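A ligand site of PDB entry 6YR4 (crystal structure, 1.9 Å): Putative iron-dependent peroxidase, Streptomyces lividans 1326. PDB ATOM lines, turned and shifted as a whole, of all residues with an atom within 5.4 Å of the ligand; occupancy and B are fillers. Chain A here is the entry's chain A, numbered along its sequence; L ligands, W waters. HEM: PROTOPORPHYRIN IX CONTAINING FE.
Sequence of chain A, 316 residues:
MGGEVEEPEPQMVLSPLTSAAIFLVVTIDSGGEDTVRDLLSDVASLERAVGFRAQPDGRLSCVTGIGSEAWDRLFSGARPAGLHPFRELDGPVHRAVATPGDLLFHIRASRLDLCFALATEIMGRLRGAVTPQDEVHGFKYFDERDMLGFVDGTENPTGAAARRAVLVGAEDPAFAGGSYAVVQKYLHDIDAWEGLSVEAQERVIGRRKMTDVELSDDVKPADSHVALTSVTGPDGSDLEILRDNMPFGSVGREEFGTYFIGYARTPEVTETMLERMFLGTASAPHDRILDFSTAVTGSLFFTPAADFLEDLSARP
O1A of the ligand sits at hydrogen-bond distance from N of Gly 153.
The guanidinium group (NH1) of Arg 243 is in salt-bridge range of an oxygen (O1A) of the ligand, 2.8 Å away.
An iron atom (FE) of the ligand is bound by a ring nitrogen (NE2) of His 225 (2.1 Å).
An oxygen (O2A) of the ligand is in hydrogen-bond range of the backbone NH (N) of Glu 155 (2.9 Å).
An oxygen (O1A) of the ligand lies within hydrogen-bond range of the backbone NH of Thr 154, at 3.3 Å.
The side-chain carboxylate (OD1) of Asp 212 is in salt-bridge range of the guanidinium group (NE) of Arg 207 (2.8 Å).
OG of Ser 293 is in hydrogen-bond range of O of Ile 289, 2.7 Å away.
The guanidinium group (NH1) of Arg 207 is in salt-bridge range of the side-chain carboxylate (OE1) of Glu 214, at 3.7 Å.
The backbone NH (N) of Phe 260 lies within hydrogen-bond range of the backbone carbonyl oxygen (O) of Gln 184 (2.9 Å).
NH1 of Arg 243 lies within salt-bridge range of OD1 of Asp 152 (3.7 Å).
O of Ile 205 lies within hydrogen-bond range of N of Val 226 (2.9 Å).
O of Val 226 sits at hydrogen-bond distance from OG of Ser 230 (2.5 Å).
The backbone carbonyl oxygen (O) of Arg 243 lies within hydrogen-bond range of the side-chain amide nitrogen (ND2) of Asn 156 (2.8 Å).
Residues that only touch the ligand: Asp 146 (3.4 Å), Leu 148 (3.9 Å), Phe 150 (3.6 Å), Val 151 (3.4 Å), Asp 152 (3.3 Å), Gln 184 (3.3 Å), Tyr 186 (3.3 Å), His 188 (3.7 Å), Ile 205 (3.9 Å), Arg 207 (3.4 Å), Val 226 (3.5 Å), Thr 229 (3.2 Å), Ser 230 (3.6 Å), Asn 245 (3.9 Å), Thr 258 (3.6 Å), Phe 260 (3.4 Å), Thr 270 (3.8 Å), Met 273 (3.8 Å), Leu 274 (3.7 Å), Met 277 (3.6 Å), Ile 289 (3.6 Å) and Ser 293 (3.98 Å).
Hydrophobic or aromatic side chains within 4 Å of the ligand: Leu 148, Phe 150, Tyr 186, His 188, Ile 205, His 225, Val 226, Phe 260, Met 273, Leu 274, Met 277 and Ile 289.
27 residues have an atom within 4 Å of the ligand: Asp 146, Leu 148, Phe 150, Val 151, Asp 152, Gly 153, Thr 154, Glu 155, Gln 184, Tyr 186, His 188, Ile 205, Arg 207, His 225, Val 226, Thr 229, Ser 230, Arg 243, Asn 245, Thr 258, Phe 260, Thr 270, Met 273, Leu 274, Met 277, Ile 289 and Ser 293.
The nearest printed residue that does not touch the ligand is Ile 241 (4.1 Å).
Water W4 lies within hydrogen-bond range of an oxygen (O2D) of the ligand (2.6 Å), the side-chain carboxylate of Glu 214 (2.9 Å) and the side-chain carboxylate of Glu 155 (3.2 Å).
Water W1 bridges O2D of the ligand (2.7 Å) and NH1 of Arg 207 (2.9 Å).
Water W3 bridges O1D of the ligand (2.8 Å) and OG of Ser 230 (3.3 Å).
Water W2 lies within hydrogen-bond range of O of Thr 229 and O1D of the ligand.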
ATOM      1  N   ASP A 146       7.412  -9.178  28.912  1.00  0.00           N
ATOM      2  CA  ASP A 146       7.043  -9.052  27.480  1.00  0.00           C
ATOM      3  C   ASP A 146       7.278  -7.609  27.042  1.00  0.00           C
ATOM      4  O   ASP A 146       7.692  -6.791  27.870  1.00  0.00           O
ATOM      5  CB  ASP A 146       5.627  -9.561  27.217  1.00  0.00           C
ATOM      6  CG  ASP A 146       4.548  -8.959  28.087  1.00  0.00           C
ATOM      7  OD1 ASP A 146       4.662  -7.742  28.369  1.00  0.00           O
ATOM      8  OD2 ASP A 146       3.621  -9.715  28.476  1.00  0.00           O
ATOM      9  N   LEU A 148       5.133  -5.471  26.480  1.00  0.00           N
ATOM     10  CA  LEU A 148       4.230  -4.546  27.224  1.00  0.00           C
ATOM     11  C   LEU A 148       4.817  -4.208  28.586  1.00  0.00           C
ATOM     12  O   LEU A 148       4.196  -3.372  29.273  1.00  0.00           O
ATOM     13  CB  LEU A 148       2.842  -5.164  27.351  1.00  0.00           C
ATOM     14  CG  LEU A 148       2.152  -5.517  26.042  1.00  0.00           C
ATOM     15  CD1 LEU A 148       0.772  -6.109  26.303  1.00  0.00           C
ATOM     16  CD2 LEU A 148       2.058  -4.308  25.099  1.00  0.00           C
ATOM     17  N   PHE A 150       5.251  -6.267  31.179  1.00  0.00           N
ATOM     18  CA  PHE A 150       4.651  -7.110  32.249  1.00  0.00           C
ATOM     19  C   PHE A 150       5.375  -8.458  32.292  1.00  0.00           C
ATOM     20  O   PHE A 150       5.811  -8.944  31.236  1.00  0.00           O
ATOM     21  CB  PHE A 150       3.147  -7.292  32.032  1.00  0.00           C
ATOM     22  CG  PHE A 150       2.333  -6.102  32.473  1.00  0.00           C
ATOM     23  CD1 PHE A 150       2.357  -4.931  31.747  1.00  0.00           C
ATOM     24  CD2 PHE A 150       1.646  -6.131  33.676  1.00  0.00           C
ATOM     25  CE1 PHE A 150       1.644  -3.822  32.177  1.00  0.00           C
ATOM     26  CE2 PHE A 150       0.919  -5.041  34.084  1.00  0.00           C
ATOM     27  CZ  PHE A 150       0.908  -3.884  33.334  1.00  0.00           C
ATOM     28  N   VAL A 151       5.462  -9.033  33.482  1.00  0.00           N
ATOM     29  CA  VAL A 151       6.020 -10.406  33.647  1.00  0.00           C
ATOM     30  C   VAL A 151       5.054 -11.365  32.959  1.00  0.00           C
ATOM     31  O   VAL A 151       3.842 -11.246  33.168  1.00  0.00           O
ATOM     32  CB  VAL A 151       6.256 -10.774  35.121  1.00  0.00           C
ATOM     33  CG1 VAL A 151       6.726 -12.200  35.243  1.00  0.00           C
ATOM     34  CG2 VAL A 151       7.212  -9.785  35.792  1.00  0.00           C
ATOM     35  N   ASP A 152       5.591 -12.291  32.170  1.00  0.00           N
ATOM     36  CA  ASP A 152       4.795 -13.162  31.281  1.00  0.00           C
ATOM     37  C   ASP A 152       5.179 -14.614  31.597  1.00  0.00           C
ATOM     38  O   ASP A 152       6.344 -14.976  31.377  1.00  0.00           O
ATOM     39  CB  ASP A 152       5.044 -12.648  29.864  1.00  0.00           C
ATOM     40  CG  ASP A 152       4.167 -13.201  28.762  1.00  0.00           C
ATOM     41  OD1 ASP A 152       3.937 -14.443  28.779  1.00  0.00           O
ATOM     42  OD2 ASP A 152       3.755 -12.385  27.860  1.00  0.00           O
ATOM     43  N   GLY A 153       4.227 -15.419  32.095  1.00  0.00           N
ATOM     44  CA  GLY A 153       4.430 -16.839  32.433  1.00  0.00           C
ATOM     45  C   GLY A 153       4.130 -17.170  33.903  1.00  0.00           C
ATOM     46  O   GLY A 153       4.125 -18.349  34.232  1.00  0.00           O
ATOM     47  N   THR A 154       3.855 -16.171  34.731  1.00  0.00           N
ATOM     48  CA  THR A 154       3.729 -16.285  36.203  1.00  0.00           C
ATOM     49  C   THR A 154       2.740 -17.403  36.579  1.00  0.00           C
ATOM     50  O   THR A 154       3.095 -18.205  37.467  1.00  0.00           O
ATOM     51  CB  THR A 154       3.247 -14.970  36.819  1.00  0.00           C
ATOM     52  OG1 THR A 154       4.099 -13.956  36.283  1.00  0.00           O
ATOM     53  CG2 THR A 154       3.290 -15.038  38.329  1.00  0.00           C
ATOM     54  N   GLU A 155       1.554 -17.455  35.951  1.00  0.00           N
ATOM     55  CA  GLU A 155       0.464 -18.389  36.350  1.00  0.00           C
ATOM     56  C   GLU A 155       0.528 -19.681  35.532  1.00  0.00           C
ATOM     57  O   GLU A 155      -0.377 -20.492  35.696  1.00  0.00           O
ATOM     58  CB  GLU A 155      -0.884 -17.683  36.272  1.00  0.00           C
ATOM     59  CG  GLU A 155      -1.010 -16.619  37.347  1.00  0.00           C
ATOM     60  CD  GLU A 155      -0.768 -17.185  38.735  1.00  0.00           C
ATOM     61  OE1 GLU A 155      -1.609 -17.953  39.180  1.00  0.00           O
ATOM     62  OE2 GLU A 155       0.301 -16.951  39.331  1.00  0.00           O
ATOM     63  N   ASN A 156       1.575 -19.908  34.722  1.00  0.00           N
ATOM     64  CA  ASN A 156       1.769 -21.265  34.122  1.00  0.00           C
ATOM     65  C   ASN A 156       1.664 -22.339  35.192  1.00  0.00           C
ATOM     66  O   ASN A 156       2.175 -22.171  36.300  1.00  0.00           O
ATOM     67  CB  ASN A 156       3.091 -21.404  33.387  1.00  0.00           C
ATOM     68  CG  ASN A 156       2.993 -20.957  31.948  1.00  0.00           C
ATOM     69  OD1 ASN A 156       1.970 -21.227  31.300  1.00  0.00           O
ATOM     70  ND2 ASN A 156       4.026 -20.296  31.441  1.00  0.00           N
ATOM     71  N   GLN A 184       0.416 -17.779  17.719  1.00  0.00           N
ATOM     72  CA  GLN A 184      -0.034 -16.505  17.141  1.00  0.00           C
ATOM     73  C   GLN A 184       1.134 -15.539  17.324  1.00  0.00           C
ATOM     74  O   GLN A 184       1.520 -15.347  18.499  1.00  0.00           O
ATOM     75  CB  GLN A 184      -1.252 -15.944  17.874  1.00  0.00           C
ATOM     76  CG  GLN A 184      -2.531 -16.723  17.713  1.00  0.00           C
ATOM     77  CD  GLN A 184      -3.625 -16.026  18.486  1.00  0.00           C
ATOM     78  OE1 GLN A 184      -3.530 -15.813  19.700  1.00  0.00           O
ATOM     79  NE2 GLN A 184      -4.674 -15.603  17.780  1.00  0.00           N
ATOM     80  N   TYR A 186       2.087 -11.916  17.532  1.00  0.00           N
ATOM     81  CA  TYR A 186       1.459 -10.625  17.889  1.00  0.00           C
ATOM     82  C   TYR A 186       2.477  -9.499  17.712  1.00  0.00           C
ATOM     83  O   TYR A 186       3.633  -9.629  18.133  1.00  0.00           O
ATOM     84  CB  TYR A 186       0.926 -10.648  19.302  1.00  0.00           C
ATOM     85  CG  TYR A 186      -0.364 -11.398  19.516  1.00  0.00           C
ATOM     86  CD1 TYR A 186      -1.581 -10.788  19.272  1.00  0.00           C
ATOM     87  CD2 TYR A 186      -0.368 -12.708  19.974  1.00  0.00           C
ATOM     88  CE1 TYR A 186      -2.779 -11.445  19.494  1.00  0.00           C
ATOM     89  CE2 TYR A 186      -1.564 -13.395  20.189  1.00  0.00           C
ATOM     90  CZ  TYR A 186      -2.772 -12.750  19.971  1.00  0.00           C
ATOM     91  OH  TYR A 186      -3.947 -13.372  20.183  1.00  0.00           O
ATOM     92  N   HIS A 188       2.672  -5.348  18.822  1.00  0.00           N
ATOM     93  CA  HIS A 188       2.085  -4.424  19.824  1.00  0.00           C
ATOM     94  C   HIS A 188       2.142  -3.003  19.277  1.00  0.00           C
ATOM     95  O   HIS A 188       3.144  -2.634  18.648  1.00  0.00           O
ATOM     96  CB  HIS A 188       2.793  -4.564  21.174  1.00  0.00           C
ATOM     97  CG  HIS A 188       2.659  -5.916  21.770  1.00  0.00           C
ATOM     98  ND1 HIS A 188       1.440  -6.383  22.222  1.00  0.00           N
ATOM     99  CD2 HIS A 188       3.572  -6.878  22.030  1.00  0.00           C
ATOM    100  CE1 HIS A 188       1.610  -7.603  22.716  1.00  0.00           C
ATOM    101  NE2 HIS A 188       2.901  -7.935  22.629  1.00  0.00           N
ATOM    102  N   ILE A 205      -4.133  -5.609  31.825  1.00  0.00           N
ATOM    103  CA  ILE A 205      -3.540  -6.964  32.022  1.00  0.00           C
ATOM    104  C   ILE A 205      -4.288  -7.696  33.148  1.00  0.00           C
ATOM    105  O   ILE A 205      -4.600  -8.887  32.951  1.00  0.00           O
ATOM    106  CB  ILE A 205      -2.034  -6.861  32.294  1.00  0.00           C
ATOM    107  CG1 ILE A 205      -1.326  -6.127  31.147  1.00  0.00           C
ATOM    108  CG2 ILE A 205      -1.423  -8.231  32.601  1.00  0.00           C
ATOM    109  CD1 ILE A 205      -1.293  -6.883  29.854  1.00  0.00           C
ATOM    110  N   ARG A 207      -2.894  -7.528  36.452  1.00  0.00           N
ATOM    111  CA  ARG A 207      -1.818  -7.726  37.456  1.00  0.00           C
ATOM    112  C   ARG A 207      -1.091  -6.408  37.590  1.00  0.00           C
ATOM    113  O   ARG A 207      -1.197  -5.594  36.671  1.00  0.00           O
ATOM    114  CB  ARG A 207      -0.827  -8.816  37.046  1.00  0.00           C
ATOM    115  CG  ARG A 207      -1.478 -10.074  36.482  1.00  0.00           C
ATOM    116  CD  ARG A 207      -0.438 -11.163  36.251  1.00  0.00           C
ATOM    117  NE  ARG A 207       0.216 -11.567  37.488  1.00  0.00           N
ATOM    118  CZ  ARG A 207      -0.239 -12.515  38.304  1.00  0.00           C
ATOM    119  NH1 ARG A 207      -1.326 -13.192  38.000  1.00  0.00           N
ATOM    120  NH2 ARG A 207       0.421 -12.800  39.418  1.00  0.00           N
ATOM    121  N   ASP A 212       4.009  -7.689  39.876  1.00  0.00           N
ATOM    122  CA  ASP A 212       3.384  -8.882  39.251  1.00  0.00           C
ATOM    123  C   ASP A 212       2.401  -9.535  40.218  1.00  0.00           C
ATOM    124  O   ASP A 212       2.237 -10.755  40.149  1.00  0.00           O
ATOM    125  CB  ASP A 212       4.438  -9.903  38.855  1.00  0.00           C
ATOM    126  CG  ASP A 212       3.924 -10.962  37.905  1.00  0.00           C
ATOM    127  OD1 ASP A 212       2.892 -10.708  37.233  1.00  0.00           O
ATOM    128  OD2 ASP A 212       4.610 -12.006  37.797  1.00  0.00           O
ATOM    129  N   GLU A 214      -1.373 -10.282  41.202  1.00  0.00           N
ATOM    130  CA  GLU A 214      -2.702 -10.294  40.532  1.00  0.00           C
ATOM    131  C   GLU A 214      -3.616  -9.260  41.206  1.00  0.00           C
ATOM    132  O   GLU A 214      -3.509  -9.107  42.429  1.00  0.00           O
ATOM    133  CB  GLU A 214      -3.302 -11.697  40.582  1.00  0.00           C
ATOM    134  CG  GLU A 214      -4.563 -11.799  39.760  1.00  0.00           C
ATOM    135  CD  GLU A 214      -5.063 -13.217  39.556  1.00  0.00           C
ATOM    136  OE1 GLU A 214      -4.326 -14.157  39.867  1.00  0.00           O
ATOM    137  OE2 GLU A 214      -6.179 -13.347  39.046  1.00  0.00           O
ATOM    138  N   HIS A 225      -6.986  -9.019  30.580  1.00  0.00           N
ATOM    139  CA  HIS A 225      -6.428 -10.260  29.973  1.00  0.00           C
ATOM    140  C   HIS A 225      -6.562 -11.411  30.974  1.00  0.00           C
ATOM    141  O   HIS A 225      -6.970 -12.519  30.591  1.00  0.00           O
ATOM    142  CB  HIS A 225      -4.972 -10.028  29.560  1.00  0.00           C
ATOM    143  CG  HIS A 225      -4.374 -11.179  28.820  1.00  0.00           C
ATOM    144  ND1 HIS A 225      -4.923 -11.648  27.652  1.00  0.00           N
ATOM    145  CD2 HIS A 225      -3.263 -11.929  29.047  1.00  0.00           C
ATOM    146  CE1 HIS A 225      -4.207 -12.656  27.189  1.00  0.00           C
ATOM    147  NE2 HIS A 225      -3.181 -12.853  28.037  1.00  0.00           N
ATOM    148  N   VAL A 226      -6.221 -11.172  32.242  1.00  0.00           N
ATOM    149  CA  VAL A 226      -6.200 -12.267  33.232  1.00  0.00           C
ATOM    150  C   VAL A 226      -7.641 -12.727  33.471  1.00  0.00           C
ATOM    151  O   VAL A 226      -7.828 -13.941  33.584  1.00  0.00           O
ATOM    152  CB  VAL A 226      -5.456 -11.884  34.520  1.00  0.00           C
ATOM    153  CG1 VAL A 226      -5.750 -12.871  35.663  1.00  0.00           C
ATOM    154  CG2 VAL A 226      -3.963 -11.790  34.270  1.00  0.00           C
ATOM    155  N   THR A 229      -8.743 -14.955  30.380  1.00  0.00           N
ATOM    156  CA  THR A 229      -7.933 -16.184  30.098  1.00  0.00           C
ATOM    157  C   THR A 229      -7.908 -17.066  31.349  1.00  0.00           C
ATOM    158  O   THR A 229      -7.200 -18.081  31.348  1.00  0.00           O
ATOM    159  CB  THR A 229      -6.537 -15.877  29.546  1.00  0.00           C
ATOM    160  OG1 THR A 229      -5.772 -15.181  30.512  1.00  0.00           O
ATOM    161  CG2 THR A 229      -6.537 -15.051  28.279  1.00  0.00           C
ATOM    162  N   SER A 230      -8.666 -16.670  32.381  1.00  0.00           N
ATOM    163  CA  SER A 230      -8.997 -17.506  33.548  1.00  0.00           C
ATOM    164  C   SER A 230     -10.310 -18.255  33.271  1.00  0.00           C
ATOM    165  O   SER A 230     -11.366 -17.588  33.083  1.00  0.00           O
ATOM    166  CB  SER A 230      -9.034 -16.675  34.801  1.00  0.00           C
ATOM    167  OG  SER A 230      -7.777 -16.053  34.993  1.00  0.00           O
ATOM    168  N   ILE A 241      -3.442 -23.916  30.425  1.00  0.00           N
ATOM    169  CA  ILE A 241      -2.530 -24.156  29.280  1.00  0.00           C
ATOM    170  C   ILE A 241      -1.115 -23.794  29.749  1.00  0.00           C
ATOM    171  O   ILE A 241      -0.990 -23.142  30.776  1.00  0.00           O
ATOM    172  CB  ILE A 241      -2.980 -23.342  28.061  1.00  0.00           C
ATOM    173  CG1 ILE A 241      -2.809 -21.837  28.248  1.00  0.00           C
ATOM    174  CG2 ILE A 241      -4.410 -23.695  27.680  1.00  0.00           C
ATOM    175  CD1 ILE A 241      -3.023 -21.086  26.985  1.00  0.00           C
ATOM    176  N   ARG A 243       2.174 -21.862  28.514  1.00  0.00           N
ATOM    177  CA  ARG A 243       2.609 -20.859  27.509  1.00  0.00           C
ATOM    178  C   ARG A 243       4.104 -20.670  27.609  1.00  0.00           C
ATOM    179  O   ARG A 243       4.656 -20.797  28.737  1.00  0.00           O
ATOM    180  CB  ARG A 243       1.919 -19.524  27.779  1.00  0.00           C
ATOM    181  CG  ARG A 243       0.405 -19.580  27.666  1.00  0.00           C
ATOM    182  CD  ARG A 243      -0.198 -18.337  28.310  1.00  0.00           C
ATOM    183  NE  ARG A 243      -0.112 -18.389  29.751  1.00  0.00           N
ATOM    184  CZ  ARG A 243       0.480 -17.489  30.540  1.00  0.00           C
ATOM    185  NH1 ARG A 243       0.986 -16.355  30.075  1.00  0.00           N
ATOM    186  NH2 ARG A 243       0.468 -17.718  31.846  1.00  0.00           N
ATOM    187  N   ASN A 245       5.602 -17.680  25.891  1.00  0.00           N
ATOM    188  CA  ASN A 245       5.548 -16.451  25.049  1.00  0.00           C
ATOM    189  C   ASN A 245       6.944 -15.873  24.920  1.00  0.00           C
ATOM    190  O   ASN A 245       7.679 -15.863  25.899  1.00  0.00           O
ATOM    191  CB  ASN A 245       4.595 -15.399  25.625  1.00  0.00           C
ATOM    192  CG  ASN A 245       3.178 -15.904  25.658  1.00  0.00           C
ATOM    193  OD1 ASN A 245       2.886 -16.935  25.062  1.00  0.00           O
ATOM    194  ND2 ASN A 245       2.316 -15.213  26.401  1.00  0.00           N
ATOM    195  N   THR A 258       5.012 -10.047  20.615  1.00  0.00           N
ATOM    196  CA  THR A 258       4.923 -11.218  21.507  1.00  0.00           C
ATOM    197  C   THR A 258       4.669 -12.406  20.605  1.00  0.00           C
ATOM    198  O   THR A 258       3.619 -12.466  19.946  1.00  0.00           O
ATOM    199  CB  THR A 258       3.870 -11.067  22.600  1.00  0.00           C
ATOM    200  OG1 THR A 258       4.240 -10.011  23.496  1.00  0.00           O
ATOM    201  CG2 THR A 258       3.740 -12.367  23.350  1.00  0.00           C
ATOM    202  N   PHE A 260       3.189 -15.658  20.826  1.00  0.00           N
ATOM    203  CA  PHE A 260       2.322 -16.465  21.707  1.00  0.00           C
ATOM    204  C   PHE A 260       2.419 -17.915  21.282  1.00  0.00           C
ATOM    205  O   PHE A 260       2.226 -18.233  20.077  1.00  0.00           O
ATOM    206  CB  PHE A 260       0.846 -16.056  21.644  1.00  0.00           C
ATOM    207  CG  PHE A 260       0.001 -17.020  22.414  1.00  0.00           C
ATOM    208  CD1 PHE A 260      -0.061 -16.957  23.793  1.00  0.00           C
ATOM    209  CD2 PHE A 260      -0.672 -18.038  21.766  1.00  0.00           C
ATOM    210  CE1 PHE A 260      -0.794 -17.879  24.519  1.00  0.00           C
ATOM    211  CE2 PHE A 260      -1.394 -18.988  22.494  1.00  0.00           C
ATOM    212  CZ  PHE A 260      -1.483 -18.883  23.865  1.00  0.00           C
ATOM    213  N   THR A 270      -7.572 -23.900  24.861  1.00  0.00           N
ATOM    214  CA  THR A 270      -6.898 -22.743  24.230  1.00  0.00           C
ATOM    215  C   THR A 270      -7.880 -21.904  23.425  1.00  0.00           C
ATOM    216  O   THR A 270      -7.841 -20.670  23.522  1.00  0.00           O
ATOM    217  CB  THR A 270      -5.757 -23.224  23.334  1.00  0.00           C
ATOM    218  OG1 THR A 270      -4.986 -24.143  24.098  1.00  0.00           O
ATOM    219  CG2 THR A 270      -4.905 -22.060  22.888  1.00  0.00           C
ATOM    220  N   MET A 273     -10.233 -19.804  25.515  1.00  0.00           N
ATOM    221  CA  MET A 273      -9.535 -18.541  25.911  1.00  0.00           C
ATOM    222  C   MET A 273      -9.569 -17.568  24.727  1.00  0.00           C
ATOM    223  O   MET A 273      -9.929 -16.403  24.933  1.00  0.00           O
ATOM    224  CB  MET A 273      -8.100 -18.850  26.347  1.00  0.00           C
ATOM    225  CG  MET A 273      -8.063 -19.661  27.603  1.00  0.00           C
ATOM    226  SD  MET A 273      -6.397 -20.233  28.047  1.00  0.00           S
ATOM    227  CE  MET A 273      -6.758 -20.953  29.645  1.00  0.00           C
ATOM    228  N   LEU A 274      -9.264 -18.041  23.527  1.00  0.00           N
ATOM    229  CA  LEU A 274      -9.300 -17.221  22.289  1.00  0.00           C
ATOM    230  C   LEU A 274     -10.705 -16.635  22.053  1.00  0.00           C
ATOM    231  O   LEU A 274     -10.801 -15.431  21.766  1.00  0.00           O
ATOM    232  CB  LEU A 274      -8.810 -18.063  21.114  1.00  0.00           C
ATOM    233  CG  LEU A 274      -7.300 -18.251  21.098  1.00  0.00           C
ATOM    234  CD1 LEU A 274      -6.885 -19.289  20.084  1.00  0.00           C
ATOM    235  CD2 LEU A 274      -6.609 -16.925  20.808  1.00  0.00           C
ATOM    236  N   MET A 277     -11.361 -13.857  24.457  1.00  0.00           N
ATOM    237  CA  MET A 277     -10.499 -12.702  24.107  1.00  0.00           C
ATOM    238  C   MET A 277     -11.085 -11.941  22.919  1.00  0.00           C
ATOM    239  O   MET A 277     -11.239 -10.721  23.018  1.00  0.00           O
ATOM    240  CB  MET A 277      -9.089 -13.186  23.771  1.00  0.00           C
ATOM    241  CG  MET A 277      -8.313 -13.651  24.962  1.00  0.00           C
ATOM    242  SD  MET A 277      -6.665 -14.245  24.629  1.00  0.00           S
ATOM    243  CE  MET A 277      -5.898 -12.782  23.935  1.00  0.00           C
ATOM    244  N   ILE A 289      -6.225  -6.322  26.047  1.00  0.00           N
ATOM    245  CA  ILE A 289      -4.858  -6.500  25.501  1.00  0.00           C
ATOM    246  C   ILE A 289      -4.878  -6.426  23.973  1.00  0.00           C
ATOM    247  O   ILE A 289      -3.828  -6.049  23.427  1.00  0.00           O
ATOM    248  CB  ILE A 289      -4.234  -7.810  26.003  1.00  0.00           C
ATOM    249  CG1 ILE A 289      -2.728  -7.636  26.166  1.00  0.00           C
ATOM    250  CG2 ILE A 289      -4.606  -9.001  25.124  1.00  0.00           C
ATOM    251  CD1 ILE A 289      -2.068  -8.779  26.893  1.00  0.00           C
ATOM    252  N   LEU A 290      -5.992  -6.784  23.325  1.00  0.00           N
ATOM    253  CA  LEU A 290      -6.096  -6.793  21.851  1.00  0.00           C
ATOM    254  C   LEU A 290      -6.230  -5.374  21.324  1.00  0.00           C
ATOM    255  O   LEU A 290      -6.002  -5.169  20.113  1.00  0.00           O
ATOM    256  CB  LEU A 290      -7.295  -7.655  21.430  1.00  0.00           C
ATOM    257  CG  LEU A 290      -7.123  -9.147  21.731  1.00  0.00           C
ATOM    258  CD1 LEU A 290      -8.390  -9.938  21.369  1.00  0.00           C
ATOM    259  CD2 LEU A 290      -5.897  -9.710  21.020  1.00  0.00           C
ATOM    260  N   SER A 293      -2.534  -5.017  20.665  1.00  0.00           N
ATOM    261  CA  SER A 293      -1.913  -6.264  20.170  1.00  0.00           C
ATOM    262  C   SER A 293      -2.674  -6.751  18.941  1.00  0.00           C
ATOM    263  O   SER A 293      -3.862  -7.033  19.104  1.00  0.00           O
ATOM    264  CB  SER A 293      -1.920  -7.327  21.237  1.00  0.00           C
ATOM    265  OG  SER A 293      -1.433  -6.868  22.495  1.00  0.00           O
HETATM  266  CHA HEM L   1      -1.411 -14.397  31.376  1.00  0.00           C
HETATM  267  CHB HEM L   1       0.630 -11.480  28.148  1.00  0.00           C
HETATM  268  CHC HEM L   1      -1.867 -13.611  24.596  1.00  0.00           C
HETATM  269  CHD HEM L   1      -3.388 -16.885  27.789  1.00  0.00           C
HETATM  270  C1A HEM L   1      -0.703 -13.384  30.809  1.00  0.00           C
HETATM  271  C2A HEM L   1      -0.004 -12.421  31.565  1.00  0.00           C
HETATM  272  C3A HEM L   1       0.587 -11.559  30.669  1.00  0.00           C
HETATM  273  C4A HEM L   1       0.258 -12.034  29.358  1.00  0.00           C
HETATM  274  CMA HEM L   1       1.434 -10.342  30.996  1.00  0.00           C
HETATM  275  CAA HEM L   1       0.005 -12.398  33.086  1.00  0.00           C
HETATM  276  CBA HEM L   1       1.145 -13.227  33.675  1.00  0.00           C
HETATM  277  CGA HEM L   1       1.017 -14.693  33.498  1.00  0.00           C
HETATM  278  O1A HEM L   1       1.588 -15.169  32.503  1.00  0.00           O
HETATM  279  O2A HEM L   1       0.382 -15.413  34.320  1.00  0.00           O
HETATM  280  C1B HEM L   1       0.129 -11.817  26.903  1.00  0.00           C
HETATM  281  C2B HEM L   1       0.430 -11.074  25.745  1.00  0.00           C
HETATM  282  C3B HEM L   1      -0.235 -11.641  24.710  1.00  0.00           C
HETATM  283  C4B HEM L   1      -1.040 -12.753  25.295  1.00  0.00           C
HETATM  284  CMB HEM L   1       1.365  -9.901  25.595  1.00  0.00           C
HETATM  285  CAB HEM L   1      -0.241 -11.045  23.376  1.00  0.00           C
HETATM  286  CBB HEM L   1      -1.357 -10.991  22.684  1.00  0.00           C
HETATM  287  C1C HEM L   1      -2.518 -14.713  25.149  1.00  0.00           C
HETATM  288  C2C HEM L   1      -3.332 -15.622  24.455  1.00  0.00           C
HETATM  289  C3C HEM L   1      -3.806 -16.540  25.371  1.00  0.00           C
HETATM  290  C4C HEM L   1      -3.208 -16.192  26.635  1.00  0.00           C
HETATM  291  CMC HEM L   1      -3.622 -15.556  22.992  1.00  0.00           C
HETATM  292  CAC HEM L   1      -4.651 -17.747  25.187  1.00  0.00           C
HETATM  293  CBC HEM L   1      -4.988 -18.242  24.025  1.00  0.00           C
HETATM  294  C1D HEM L   1      -2.945 -16.436  29.023  1.00  0.00           C
HETATM  295  C2D HEM L   1      -3.255 -17.192  30.236  1.00  0.00           C
HETATM  296  C3D HEM L   1      -2.752 -16.480  31.251  1.00  0.00           C
HETATM  297  C4D HEM L   1      -2.115 -15.311  30.617  1.00  0.00           C
HETATM  298  CMD HEM L   1      -4.023 -18.472  30.371  1.00  0.00           C
HETATM  299  CAD HEM L   1      -2.837 -16.833  32.713  1.00  0.00           C
HETATM  300  CBD HEM L   1      -4.082 -16.189  33.323  1.00  0.00           C
HETATM  301  CGD HEM L   1      -4.236 -16.662  34.766  1.00  0.00           C
HETATM  302  O1D HEM L   1      -4.643 -17.848  34.976  1.00  0.00           O
HETATM  303  O2D HEM L   1      -4.027 -15.927  35.739  1.00  0.00           O
HETATM  304  NA  HEM L   1      -0.525 -13.135  29.476  1.00  0.00           N
HETATM  305  NB  HEM L   1      -0.749 -12.759  26.611  1.00  0.00           N
HETATM  306  NC  HEM L   1      -2.472 -15.054  26.466  1.00  0.00           N
HETATM  307  ND  HEM L   1      -2.223 -15.331  29.287  1.00  0.00           N
HETATM  308 FE   HEM L   1      -1.491 -14.092  28.021  1.00  0.00          FE
HETATM  309  O   HOH W   1      -1.905 -14.219  35.401  1.00  0.00           O
HETATM  310  O   HOH W   2      -5.515 -19.558  32.895  1.00  0.00           O
HETATM  311  O   HOH W   3      -6.595 -18.470  36.841  1.00  0.00           O
HETATM  312  O   HOH W   4      -4.348 -16.524  38.216  1.00  0.00           O
